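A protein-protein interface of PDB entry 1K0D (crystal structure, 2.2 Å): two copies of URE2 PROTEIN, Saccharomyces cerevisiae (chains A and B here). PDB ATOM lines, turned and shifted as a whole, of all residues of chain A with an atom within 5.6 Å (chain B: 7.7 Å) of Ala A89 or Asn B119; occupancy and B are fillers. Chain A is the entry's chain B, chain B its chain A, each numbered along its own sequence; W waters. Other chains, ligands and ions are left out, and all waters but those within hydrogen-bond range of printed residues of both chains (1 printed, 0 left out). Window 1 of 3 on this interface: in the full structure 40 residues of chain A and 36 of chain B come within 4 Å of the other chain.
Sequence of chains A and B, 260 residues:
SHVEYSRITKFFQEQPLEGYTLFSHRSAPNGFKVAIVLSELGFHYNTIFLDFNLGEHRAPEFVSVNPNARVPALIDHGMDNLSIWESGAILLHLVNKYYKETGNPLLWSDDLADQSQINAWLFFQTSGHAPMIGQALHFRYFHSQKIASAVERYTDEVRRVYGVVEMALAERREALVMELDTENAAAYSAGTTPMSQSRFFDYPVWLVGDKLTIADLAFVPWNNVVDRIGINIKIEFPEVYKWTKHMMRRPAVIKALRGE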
ATOM      1  N   ILE A  84     -10.271  -2.661   1.310  1.00  0.00           N
ATOM      2  CA  ILE A  84      -9.604  -3.089   0.086  1.00  0.00           C
ATOM      3  C   ILE A  84      -9.667  -4.615   0.027  1.00  0.00           C
ATOM      4  O   ILE A  84      -9.325  -5.296   0.999  1.00  0.00           O
ATOM      5  CB  ILE A  84      -8.115  -2.660   0.033  1.00  0.00           C
ATOM      6  CG1 ILE A  84      -7.959  -1.176   0.382  1.00  0.00           C
ATOM      7  CG2 ILE A  84      -7.572  -2.883  -1.370  1.00  0.00           C
ATOM      8  CD1 ILE A  84      -7.781  -0.895   1.871  1.00  0.00           C
ATOM      9  N   TRP A  85     -10.129  -5.151  -1.098  1.00  0.00           N
ATOM     10  CA  TRP A  85     -10.226  -6.596  -1.268  1.00  0.00           C
ATOM     11  C   TRP A  85      -9.379  -6.984  -2.479  1.00  0.00           C
ATOM     12  O   TRP A  85      -9.046  -6.124  -3.292  1.00  0.00           O
ATOM     13  CB  TRP A  85     -11.689  -7.023  -1.428  1.00  0.00           C
ATOM     14  CG  TRP A  85     -12.465  -6.190  -2.388  1.00  0.00           C
ATOM     15  CD1 TRP A  85     -12.842  -4.888  -2.227  1.00  0.00           C
ATOM     16  CD2 TRP A  85     -12.951  -6.595  -3.668  1.00  0.00           C
ATOM     17  NE1 TRP A  85     -13.538  -4.456  -3.333  1.00  0.00           N
ATOM     18  CE2 TRP A  85     -13.619  -5.486  -4.232  1.00  0.00           C
ATOM     19  CE3 TRP A  85     -12.888  -7.793  -4.396  1.00  0.00           C
ATOM     20  CZ2 TRP A  85     -14.222  -5.535  -5.494  1.00  0.00           C
ATOM     21  CZ3 TRP A  85     -13.491  -7.844  -5.652  1.00  0.00           C
ATOM     22  CH2 TRP A  85     -14.149  -6.720  -6.186  1.00  0.00           C
ATOM     23  N   GLU A  86      -9.044  -8.269  -2.587  1.00  0.00           N
ATOM     24  CA  GLU A  86      -8.157  -8.811  -3.631  1.00  0.00           C
ATOM     25  C   GLU A  86      -6.737  -8.581  -3.099  1.00  0.00           C
ATOM     26  O   GLU A  86      -6.315  -7.442  -2.920  1.00  0.00           O
ATOM     27  CB  GLU A  86      -8.329  -8.100  -4.980  1.00  0.00           C
ATOM     28  CG  GLU A  86      -9.548  -8.556  -5.784  1.00  0.00           C
ATOM     29  CD  GLU A  86      -9.463 -10.016  -6.230  1.00  0.00           C
ATOM     30  OE1 GLU A  86     -10.511 -10.691  -6.228  1.00  0.00           O
ATOM     31  OE2 GLU A  86      -8.359 -10.490  -6.595  1.00  0.00           O
ATOM     32  N   SER A  87      -6.014  -9.666  -2.829  1.00  0.00           N
ATOM     33  CA  SER A  87      -4.661  -9.575  -2.289  1.00  0.00           C
ATOM     34  C   SER A  87      -3.724  -8.683  -3.116  1.00  0.00           C
ATOM     35  O   SER A  87      -2.858  -7.989  -2.564  1.00  0.00           O
ATOM     36  CB  SER A  87      -4.062 -10.976  -2.157  1.00  0.00           C
ATOM     37  OG  SER A  87      -3.999 -11.636  -3.411  1.00  0.00           O
ATOM     38  N   GLY A  88      -3.895  -8.713  -4.435  1.00  0.00           N
ATOM     39  CA  GLY A  88      -3.070  -7.895  -5.308  1.00  0.00           C
ATOM     40  C   GLY A  88      -3.301  -6.413  -5.081  1.00  0.00           C
ATOM     41  O   GLY A  88      -2.358  -5.615  -5.081  1.00  0.00           O
ATOM     42  N   ALA A  89      -4.558  -6.034  -4.877  1.00  0.00           N
ATOM     43  CA  ALA A  89      -4.883  -4.626  -4.649  1.00  0.00           C
ATOM     44  C   ALA A  89      -4.436  -4.224  -3.245  1.00  0.00           C
ATOM     45  O   ALA A  89      -4.005  -3.092  -3.020  1.00  0.00           O
ATOM     46  CB  ALA A  89      -6.398  -4.387  -4.822  1.00  0.00           C
ATOM     47  N   ILE A  90      -4.549  -5.149  -2.296  1.00  0.00           N
ATOM     48  CA  ILE A  90      -4.127  -4.857  -0.930  1.00  0.00           C
ATOM     49  C   ILE A  90      -2.617  -4.559  -0.898  1.00  0.00           C
ATOM     50  O   ILE A  90      -2.189  -3.594  -0.262  1.00  0.00           O
ATOM     51  CB  ILE A  90      -4.470  -6.039   0.031  1.00  0.00           C
ATOM     52  CG1 ILE A  90      -5.994  -6.151   0.188  1.00  0.00           C
ATOM     53  CG2 ILE A  90      -3.849  -5.810   1.404  1.00  0.00           C
ATOM     54  CD1 ILE A  90      -6.445  -7.361   0.974  1.00  0.00           C
ATOM     55  N   LEU A  91      -1.821  -5.364  -1.604  1.00  0.00           N
ATOM     56  CA  LEU A  91      -0.372  -5.160  -1.635  1.00  0.00           C
ATOM     57  C   LEU A  91       0.000  -3.808  -2.211  1.00  0.00           C
ATOM     58  O   LEU A  91       0.842  -3.098  -1.643  1.00  0.00           O
ATOM     59  CB  LEU A  91       0.341  -6.259  -2.439  1.00  0.00           C
ATOM     60  CG  LEU A  91       0.253  -7.696  -1.914  1.00  0.00           C
ATOM     61  CD1 LEU A  91       1.399  -8.521  -2.496  1.00  0.00           C
ATOM     62  CD2 LEU A  91       0.304  -7.699  -0.395  1.00  0.00           C
ATOM     63  N   LEU A  92      -0.620  -3.445  -3.334  1.00  0.00           N
ATOM     64  CA  LEU A  92      -0.330  -2.159  -3.949  1.00  0.00           C
ATOM     65  C   LEU A  92      -0.754  -1.024  -3.020  1.00  0.00           C
ATOM     66  O   LEU A  92      -0.105   0.010  -2.956  1.00  0.00           O
ATOM     67  CB  LEU A  92      -1.030  -2.025  -5.310  1.00  0.00           C
ATOM     68  CG  LEU A  92      -0.456  -2.895  -6.436  1.00  0.00           C
ATOM     69  CD1 LEU A  92      -1.154  -2.548  -7.747  1.00  0.00           C
ATOM     70  CD2 LEU A  92       1.061  -2.665  -6.565  1.00  0.00           C
ATOM     71  N   HIS A  93      -1.839  -1.218  -2.289  1.00  0.00           N
ATOM     72  CA  HIS A  93      -2.281  -0.179  -1.375  1.00  0.00           C
ATOM     73  C   HIS A  93      -1.239   0.004  -0.268  1.00  0.00           C
ATOM     74  O   HIS A  93      -0.883   1.125   0.089  1.00  0.00           O
ATOM     75  CB  HIS A  93      -3.629  -0.545  -0.762  1.00  0.00           C
ATOM     76  CG  HIS A  93      -4.189   0.521   0.126  1.00  0.00           C
ATOM     77  ND1 HIS A  93      -4.134   0.451   1.501  1.00  0.00           N
ATOM     78  CD2 HIS A  93      -4.784   1.699  -0.168  1.00  0.00           C
ATOM     79  CE1 HIS A  93      -4.672   1.542   2.015  1.00  0.00           C
ATOM     80  NE2 HIS A  93      -5.074   2.316   1.023  1.00  0.00           N
ATOM     81  N   LEU A  94      -0.743  -1.111   0.260  1.00  0.00           N
ATOM     82  CA  LEU A  94       0.250  -1.066   1.329  1.00  0.00           C
ATOM     83  C   LEU A  94       1.586  -0.432   0.940  1.00  0.00           C
ATOM     84  O   LEU A  94       2.089   0.436   1.660  1.00  0.00           O
ATOM     85  CB  LEU A  94       0.485  -2.470   1.892  1.00  0.00           C
ATOM     86  CG  LEU A  94      -0.753  -3.056   2.582  1.00  0.00           C
ATOM     87  CD1 LEU A  94      -0.412  -4.415   3.176  1.00  0.00           C
ATOM     88  CD2 LEU A  94      -1.224  -2.106   3.674  1.00  0.00           C
ATOM     89  N   GLY B  88      -3.165  -6.539 -16.815  1.00  0.00           N
ATOM     90  CA  GLY B  88      -3.371  -5.697 -15.646  1.00  0.00           C
ATOM     91  C   GLY B  88      -2.247  -4.700 -15.397  1.00  0.00           C
ATOM     92  O   GLY B  88      -2.489  -3.528 -15.094  1.00  0.00           O
ATOM     93  N   LEU B  92      -2.201  -0.484 -15.736  1.00  0.00           N
ATOM     94  CA  LEU B  92      -1.731   0.411 -14.679  1.00  0.00           C
ATOM     95  C   LEU B  92      -0.598   1.300 -15.184  1.00  0.00           C
ATOM     96  O   LEU B  92      -0.515   2.479 -14.838  1.00  0.00           O
ATOM     97  CB  LEU B  92      -1.273  -0.383 -13.451  1.00  0.00           C
ATOM     98  CG  LEU B  92      -2.425  -0.943 -12.607  1.00  0.00           C
ATOM     99  CD1 LEU B  92      -1.870  -1.682 -11.387  1.00  0.00           C
ATOM    100  CD2 LEU B  92      -3.333   0.212 -12.160  1.00  0.00           C
ATOM    101  N   VAL B  95      -2.244   4.253 -17.442  1.00  0.00           N
ATOM    102  CA  VAL B  95      -2.950   5.322 -16.731  1.00  0.00           C
ATOM    103  C   VAL B  95      -2.004   6.082 -15.810  1.00  0.00           C
ATOM    104  O   VAL B  95      -2.221   7.263 -15.526  1.00  0.00           O
ATOM    105  CB  VAL B  95      -4.159   4.795 -15.892  1.00  0.00           C
ATOM    106  CG1 VAL B  95      -5.150   4.078 -16.802  1.00  0.00           C
ATOM    107  CG2 VAL B  95      -3.681   3.870 -14.777  1.00  0.00           C
ATOM    108  N   ASN B  96      -0.971   5.401 -15.321  1.00  0.00           N
ATOM    109  CA  ASN B  96       0.006   6.066 -14.469  1.00  0.00           C
ATOM    110  C   ASN B  96       0.786   7.037 -15.339  1.00  0.00           C
ATOM    111  O   ASN B  96       0.928   8.205 -14.999  1.00  0.00           O
ATOM    112  CB  ASN B  96       0.971   5.063 -13.827  1.00  0.00           C
ATOM    113  CG  ASN B  96       0.437   4.490 -12.530  1.00  0.00           C
ATOM    114  OD1 ASN B  96       0.015   3.340 -12.470  1.00  0.00           O
ATOM    115  ND2 ASN B  96       0.444   5.299 -11.484  1.00  0.00           N
ATOM    116  N   TRP B 108      -8.686   6.759 -14.476  1.00  0.00           N
ATOM    117  CA  TRP B 108      -7.955   6.434 -13.254  1.00  0.00           C
ATOM    118  C   TRP B 108      -8.447   7.402 -12.179  1.00  0.00           C
ATOM    119  O   TRP B 108      -9.598   7.841 -12.204  1.00  0.00           O
ATOM    120  CB  TRP B 108      -6.460   6.648 -13.568  1.00  0.00           C
ATOM    121  CG  TRP B 108      -5.399   6.250 -12.558  1.00  0.00           C
ATOM    122  CD1 TRP B 108      -4.227   6.926 -12.308  1.00  0.00           C
ATOM    123  CD2 TRP B 108      -5.328   5.041 -11.784  1.00  0.00           C
ATOM    124  NE1 TRP B 108      -3.439   6.213 -11.442  1.00  0.00           N
ATOM    125  CE2 TRP B 108      -4.086   5.055 -11.102  1.00  0.00           C
ATOM    126  CE3 TRP B 108      -6.185   3.951 -11.603  1.00  0.00           C
ATOM    127  CZ2 TRP B 108      -3.686   4.019 -10.253  1.00  0.00           C
ATOM    128  CZ3 TRP B 108      -5.785   2.919 -10.758  1.00  0.00           C
ATOM    129  CH2 TRP B 108      -4.548   2.961 -10.093  1.00  0.00           C
ATOM    130  N   LEU B 112      -5.749   8.197  -3.551  1.00  0.00           N
ATOM    131  CA  LEU B 112      -5.290   6.895  -3.090  1.00  0.00           C
ATOM    132  C   LEU B 112      -6.435   5.917  -2.841  1.00  0.00           C
ATOM    133  O   LEU B 112      -6.385   4.774  -3.296  1.00  0.00           O
ATOM    134  CB  LEU B 112      -4.456   7.059  -1.816  1.00  0.00           C
ATOM    135  CG  LEU B 112      -3.673   5.826  -1.358  1.00  0.00           C
ATOM    136  CD1 LEU B 112      -2.733   5.389  -2.480  1.00  0.00           C
ATOM    137  CD2 LEU B 112      -2.882   6.138  -0.081  1.00  0.00           C
ATOM    138  N   ALA B 113      -7.460   6.364  -2.118  1.00  0.00           N
ATOM    139  CA  ALA B 113      -8.619   5.522  -1.823  1.00  0.00           C
ATOM    140  C   ALA B 113      -9.247   4.984  -3.111  1.00  0.00           C
ATOM    141  O   ALA B 113      -9.459   3.776  -3.247  1.00  0.00           O
ATOM    142  CB  ALA B 113      -9.655   6.309  -1.023  1.00  0.00           C
ATOM    143  N   ASP B 114      -9.535   5.884  -4.050  1.00  0.00           N
ATOM    144  CA  ASP B 114     -10.132   5.496  -5.332  1.00  0.00           C
ATOM    145  C   ASP B 114      -9.274   4.491  -6.084  1.00  0.00           C
ATOM    146  O   ASP B 114      -9.795   3.545  -6.680  1.00  0.00           O
ATOM    147  CB  ASP B 114     -10.339   6.721  -6.228  1.00  0.00           C
ATOM    148  CG  ASP B 114     -11.609   7.483  -5.898  1.00  0.00           C
ATOM    149  OD1 ASP B 114     -11.820   8.567  -6.491  1.00  0.00           O
ATOM    150  OD2 ASP B 114     -12.397   6.993  -5.057  1.00  0.00           O
ATOM    151  N   GLN B 115      -7.964   4.707  -6.080  1.00  0.00           N
ATOM    152  CA  GLN B 115      -7.062   3.801  -6.779  1.00  0.00           C
ATOM    153  C   GLN B 115      -7.141   2.389  -6.208  1.00  0.00           C
ATOM    154  O   GLN B 115      -7.078   1.413  -6.953  1.00  0.00           O
ATOM    155  CB  GLN B 115      -5.619   4.321  -6.719  1.00  0.00           C
ATOM    156  CG  GLN B 115      -5.414   5.588  -7.531  1.00  0.00           C
ATOM    157  CD  GLN B 115      -4.034   6.183  -7.384  1.00  0.00           C
ATOM    158  OE1 GLN B 115      -3.758   7.274  -7.899  1.00  0.00           O
ATOM    159  NE2 GLN B 115      -3.151   5.475  -6.684  1.00  0.00           N
ATOM    160  N   SER B 116      -7.298   2.280  -4.893  1.00  0.00           N
ATOM    161  CA  SER B 116      -7.381   0.967  -4.262  1.00  0.00           C
ATOM    162  C   SER B 116      -8.648   0.254  -4.717  1.00  0.00           C
ATOM    163  O   SER B 116      -8.651  -0.961  -4.871  1.00  0.00           O
ATOM    164  CB  SER B 116      -7.377   1.081  -2.731  1.00  0.00           C
ATOM    165  OG  SER B 116      -8.642   1.496  -2.230  1.00  0.00           O
ATOM    166  N   GLN B 117      -9.723   1.006  -4.933  1.00  0.00           N
ATOM    167  CA  GLN B 117     -10.969   0.392  -5.381  1.00  0.00           C
ATOM    168  C   GLN B 117     -10.828  -0.027  -6.842  1.00  0.00           C
ATOM    169  O   GLN B 117     -11.284  -1.100  -7.235  1.00  0.00           O
ATOM    170  CB  GLN B 117     -12.143   1.354  -5.217  1.00  0.00           C
ATOM    171  CG  GLN B 117     -12.440   1.735  -3.776  1.00  0.00           C
ATOM    172  CD  GLN B 117     -12.403   0.540  -2.832  1.00  0.00           C
ATOM    173  OE1 GLN B 117     -11.333   0.121  -2.379  1.00  0.00           O
ATOM    174  NE2 GLN B 117     -13.570  -0.023  -2.541  1.00  0.00           N
ATOM    175  N   ILE B 118     -10.187   0.818  -7.647  1.00  0.00           N
ATOM    176  CA  ILE B 118      -9.988   0.485  -9.048  1.00  0.00           C
ATOM    177  C   ILE B 118      -9.155  -0.803  -9.130  1.00  0.00           C
ATOM    178  O   ILE B 118      -9.531  -1.748  -9.825  1.00  0.00           O
ATOM    179  CB  ILE B 118      -9.281   1.639  -9.807  1.00  0.00           C
ATOM    180  CG1 ILE B 118     -10.223   2.840  -9.917  1.00  0.00           C
ATOM    181  CG2 ILE B 118      -8.872   1.182 -11.192  1.00  0.00           C
ATOM    182  CD1 ILE B 118      -9.553   4.099 -10.439  1.00  0.00           C
ATOM    183  N   ASN B 119      -8.036  -0.851  -8.411  1.00  0.00           N
ATOM    184  CA  ASN B 119      -7.199  -2.049  -8.418  1.00  0.00           C
ATOM    185  C   ASN B 119      -7.981  -3.278  -7.938  1.00  0.00           C
ATOM    186  O   ASN B 119      -7.811  -4.369  -8.470  1.00  0.00           O
ATOM    187  CB  ASN B 119      -5.954  -1.842  -7.544  1.00  0.00           C
ATOM    188  CG  ASN B 119      -4.925  -0.930  -8.198  1.00  0.00           C
ATOM    189  OD1 ASN B 119      -3.881  -0.622  -7.614  1.00  0.00           O
ATOM    190  ND2 ASN B 119      -5.214  -0.496  -9.414  1.00  0.00           N
ATOM    191  N   ALA B 120      -8.827  -3.110  -6.927  1.00  0.00           N
ATOM    192  CA  ALA B 120      -9.617  -4.239  -6.434  1.00  0.00           C
ATOM    193  C   ALA B 120     -10.390  -4.863  -7.605  1.00  0.00           C
ATOM    194  O   ALA B 120     -10.255  -6.050  -7.886  1.00  0.00           O
ATOM    195  CB  ALA B 120     -10.591  -3.773  -5.332  1.00  0.00           C
ATOM    196  N   TRP B 121     -11.194  -4.054  -8.293  1.00  0.00           N
ATOM    197  CA  TRP B 121     -11.966  -4.552  -9.433  1.00  0.00           C
ATOM    198  C   TRP B 121     -11.072  -5.073 -10.556  1.00  0.00           C
ATOM    199  O   TRP B 121     -11.408  -6.054 -11.225  1.00  0.00           O
ATOM    200  CB  TRP B 121     -12.888  -3.455  -9.976  1.00  0.00           C
ATOM    201  CG  TRP B 121     -14.036  -3.169  -9.065  1.00  0.00           C
ATOM    202  CD1 TRP B 121     -14.192  -2.083  -8.245  1.00  0.00           C
ATOM    203  CD2 TRP B 121     -15.175  -4.009  -8.839  1.00  0.00           C
ATOM    204  NE1 TRP B 121     -15.364  -2.201  -7.521  1.00  0.00           N
ATOM    205  CE2 TRP B 121     -15.982  -3.373  -7.867  1.00  0.00           C
ATOM    206  CE3 TRP B 121     -15.591  -5.238  -9.363  1.00  0.00           C
ATOM    207  CZ2 TRP B 121     -17.180  -3.927  -7.409  1.00  0.00           C
ATOM    208  CZ3 TRP B 121     -16.785  -5.790  -8.909  1.00  0.00           C
ATOM    209  CH2 TRP B 121     -17.564  -5.132  -7.938  1.00  0.00           C
ATOM    210  N   LEU B 122      -9.928  -4.421 -10.752  1.00  0.00           N
ATOM    211  CA  LEU B 122      -9.002  -4.826 -11.794  1.00  0.00           C
ATOM    212  C   LEU B 122      -8.431  -6.218 -11.504  1.00  0.00           C
ATOM    213  O   LEU B 122      -8.425  -7.085 -12.377  1.00  0.00           O
ATOM    214  CB  LEU B 122      -7.874  -3.794 -11.928  1.00  0.00           C
ATOM    215  CG  LEU B 122      -6.812  -4.071 -12.994  1.00  0.00           C
ATOM    216  CD1 LEU B 122      -7.479  -4.275 -14.345  1.00  0.00           C
ATOM    217  CD2 LEU B 122      -5.823  -2.917 -13.062  1.00  0.00           C
ATOM    218  N   PHE B 123      -7.938  -6.440 -10.287  1.00  0.00           N
ATOM    219  CA  PHE B 123      -7.414  -7.758  -9.959  1.00  0.00           C
ATOM    220  C   PHE B 123      -8.552  -8.778  -9.965  1.00  0.00           C
ATOM    221  O   PHE B 123      -8.348  -9.942 -10.307  1.00  0.00           O
ATOM    222  CB  PHE B 123      -6.721  -7.763  -8.594  1.00  0.00           C
ATOM    223  CG  PHE B 123      -5.290  -7.309  -8.640  1.00  0.00           C
ATOM    224  CD1 PHE B 123      -4.962  -5.968  -8.472  1.00  0.00           C
ATOM    225  CD2 PHE B 123      -4.269  -8.228  -8.848  1.00  0.00           C
ATOM    226  CE1 PHE B 123      -3.637  -5.553  -8.506  1.00  0.00           C
ATOM    227  CE2 PHE B 123      -2.936  -7.821  -8.885  1.00  0.00           C
ATOM    228  CZ  PHE B 123      -2.618  -6.483  -8.713  1.00  0.00           C
ATOM    229  N   PHE B 124      -9.753  -8.343  -9.590  1.00  0.00           N
ATOM    230  CA  PHE B 124     -10.903  -9.248  -9.587  1.00  0.00           C
ATOM    231  C   PHE B 124     -11.185  -9.708 -11.012  1.00  0.00           C
ATOM    232  O   PHE B 124     -11.417 -10.891 -11.259  1.00  0.00           O
ATOM    233  CB  PHE B 124     -12.131  -8.541  -9.011  1.00  0.00           C
ATOM    234  CG  PHE B 124     -13.367  -9.401  -8.956  1.00  0.00           C
ATOM    235  CD1 PHE B 124     -13.310 -10.699  -8.460  1.00  0.00           C
ATOM    236  CD2 PHE B 124     -14.603  -8.885  -9.339  1.00  0.00           C
ATOM    237  CE1 PHE B 124     -14.471 -11.476  -8.340  1.00  0.00           C
ATOM    238  CE2 PHE B 124     -15.774  -9.651  -9.223  1.00  0.00           C
ATOM    239  CZ  PHE B 124     -15.708 -10.945  -8.722  1.00  0.00           C
ATOM    240  N   GLN B 125     -11.147  -8.780 -11.958  1.00  0.00           N
ATOM    241  CA  GLN B 125     -11.409  -9.141 -13.346  1.00  0.00           C
ATOM    242  C   GLN B 125     -10.340 -10.085 -13.901  1.00  0.00           C
ATOM    243  O   GLN B 125     -10.665 -11.118 -14.486  1.00  0.00           O
ATOM    244  CB  GLN B 125     -11.491  -7.885 -14.224  1.00  0.00           C
ATOM    245  CG  GLN B 125     -12.082  -8.131 -15.619  1.00  0.00           C
ATOM    246  CD  GLN B 125     -11.119  -8.837 -16.560  1.00  0.00           C
ATOM    247  OE1 GLN B 125     -11.511  -9.726 -17.324  1.00  0.00           O
ATOM    248  NE2 GLN B 125      -9.857  -8.432 -16.523  1.00  0.00           N
ATOM    249  N   THR B 126      -9.071  -9.736 -13.705  1.00  0.00           N
ATOM    250  CA  THR B 126      -7.966 -10.546 -14.221  1.00  0.00           C
ATOM    251  C   THR B 126      -7.732 -11.883 -13.521  1.00  0.00           C
ATOM    252  O   THR B 126      -7.242 -12.826 -14.139  1.00  0.00           O
ATOM    253  CB  THR B 126      -6.623  -9.770 -14.176  1.00  0.00           C
ATOM    254  OG1 THR B 126      -6.274  -9.510 -12.813  1.00  0.00           O
ATOM    255  CG2 THR B 126      -6.746  -8.442 -14.905  1.00  0.00           C
ATOM    256  N   VAL B 208     -16.326   2.542  -9.975  1.00  0.00           N
ATOM    257  CA  VAL B 208     -15.638   3.424  -9.030  1.00  0.00           C
ATOM    258  C   VAL B 208     -15.713   4.918  -9.342  1.00  0.00           C
ATOM    259  O   VAL B 208     -15.566   5.332 -10.486  1.00  0.00           O
ATOM    260  CB  VAL B 208     -14.138   3.065  -8.930  1.00  0.00           C
ATOM    261  CG1 VAL B 208     -13.444   3.971  -7.892  1.00  0.00           C
ATOM    262  CG2 VAL B 208     -13.971   1.595  -8.576  1.00  0.00           C
ATOM    263  N   THR B 213     -13.443   4.055 -15.661  1.00  0.00           N
ATOM    264  CA  THR B 213     -12.040   3.773 -15.334  1.00  0.00           C
ATOM    265  C   THR B 213     -11.620   2.434 -15.937  1.00  0.00           C
ATOM    266  O   THR B 213     -12.446   1.726 -16.511  1.00  0.00           O
ATOM    267  CB  THR B 213     -11.777   3.696 -13.811  1.00  0.00           C
ATOM    268  OG1 THR B 213     -12.370   2.503 -13.279  1.00  0.00           O
ATOM    269  CG2 THR B 213     -12.339   4.923 -13.096  1.00  0.00           C
ATOM    270  N   ILE B 214     -10.342   2.087 -15.803  1.00  0.00           N
ATOM    271  CA  ILE B 214      -9.856   0.826 -16.345  1.00  0.00           C
ATOM    272  C   ILE B 214     -10.549  -0.341 -15.651  1.00  0.00           C
ATOM    273  O   ILE B 214     -10.529  -1.460 -16.146  1.00  0.00           O
ATOM    274  CB  ILE B 214      -8.319   0.689 -16.202  1.00  0.00           C
ATOM    275  CG1 ILE B 214      -7.880   1.042 -14.774  1.00  0.00           C
ATOM    276  CG2 ILE B 214      -7.625   1.592 -17.221  1.00  0.00           C
ATOM    277  CD1 ILE B 214      -6.392   0.800 -14.502  1.00  0.00           C
ATOM    278  N   ALA B 215     -11.176  -0.074 -14.509  1.00  0.00           N
ATOM    279  CA  ALA B 215     -11.893  -1.115 -13.785  1.00  0.00           C
ATOM    280  C   ALA B 215     -13.080  -1.577 -14.638  1.00  0.00           C
ATOM    281  O   ALA B 215     -13.378  -2.770 -14.712  1.00  0.00           O
ATOM    282  CB  ALA B 215     -12.389  -0.580 -12.462  1.00  0.00           C
HETATM  283  O   HOH W   1      -4.462  -0.899  -4.489  1.00  0.00           O
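The backbone carbonyl oxygen (O) of Ala B113 sits at hydrogen-bond distance from the side-chain hydroxyl (OG) of Ser B116, 2.6 Å away. The backbone carbonyl oxygen (O) of Leu B92 sits close to the side-chain amide oxygen (OD1) of Asn B96 (2.6 Å). The backbone carbonyl oxygen of Phe B123 lies within hydrogen-bond range of the side-chain hydroxyl of Thr B126. OE1 of Gln B117 sits at hydrogen-bond distance from OG of Ser B116.
CG1 of Ile A84 touches OG of Ser B116, 3.8 Å away. Trp A85 touches Ala B120. Trp B121 touches Trp A85. Glu A86 touches Phe B123. Phe B123 touches Gly A88. Asn B119 touches Ala A89. Ala B120 touches Ala A89 (N to CB, 3.5 Å). Phe B123 touches Ala A89 (CD1 to N, 3.6 Å). Leu A92 touches Asn B119 (CD1 to OD1, 3.3 Å). Leu A92 touches Phe B123.
Of chain B, only Asn B119 (3.7 Å), Ala B120 (3.5 Å) and Phe B123 (3.6 Å) come within 4 Å of Ala A89. Of chain A, only Ala A89 (3.7 Å) and Leu A92 (3.3 Å) come within 4 Å of Asn B119. Of the printed residues of chain B, Leu A92 touches Leu B92 (3.8 Å), Asn B119 (3.3 Å) and Phe B123 (3.97 Å). Of the printed residues of chain A, Trp B121 touches Trp A85 (3.7 Å). Of the printed residues of chain B, Ile A84 touches Ser B116 (3.8 Å). Printed residues of chain A within 4 Å of Leu B92: Leu A92 (3.8 Å). The nearest residue of chain A that does not touch Asn B119 is Glu A86 (5.1 Å). The nearest printed residue of chain A that does not touch Phe B124 is Ala A89 (7.0 Å).
Of the 24 printed residues of chain B, 7 touch a printed residue of chain A. Hydrophobic or aromatic side chains of chain B within 4 Å of the printed part of chain A: Leu B92, Ala B120, Trp B121, Phe B123 and Phe B124. Along chain B the printed residues that touch a printed residue of chain A span positions 92 to 124. Of the 11 printed residues of chain A, 7 touch a printed residue of chain B. Hydrophobic or aromatic side chains of chain A within 4 Å of the printed part of chain B: Ile A84, Trp A85, Ala A89, Leu A92 and His A93. Along chain A the printed residues that touch a printed residue of chain B span positions 84 to 93.
Leu B92 touches its own counterpart, Leu A92. 2 positions are printed for both chains. Of the 15 pairs that touch across the chains among the printed residues, 1 has its exchanged pair printed and touching as well.
Water W1 lies within hydrogen-bond range of O of Ala A89, OD1 of Asn B119 and N of His A93.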
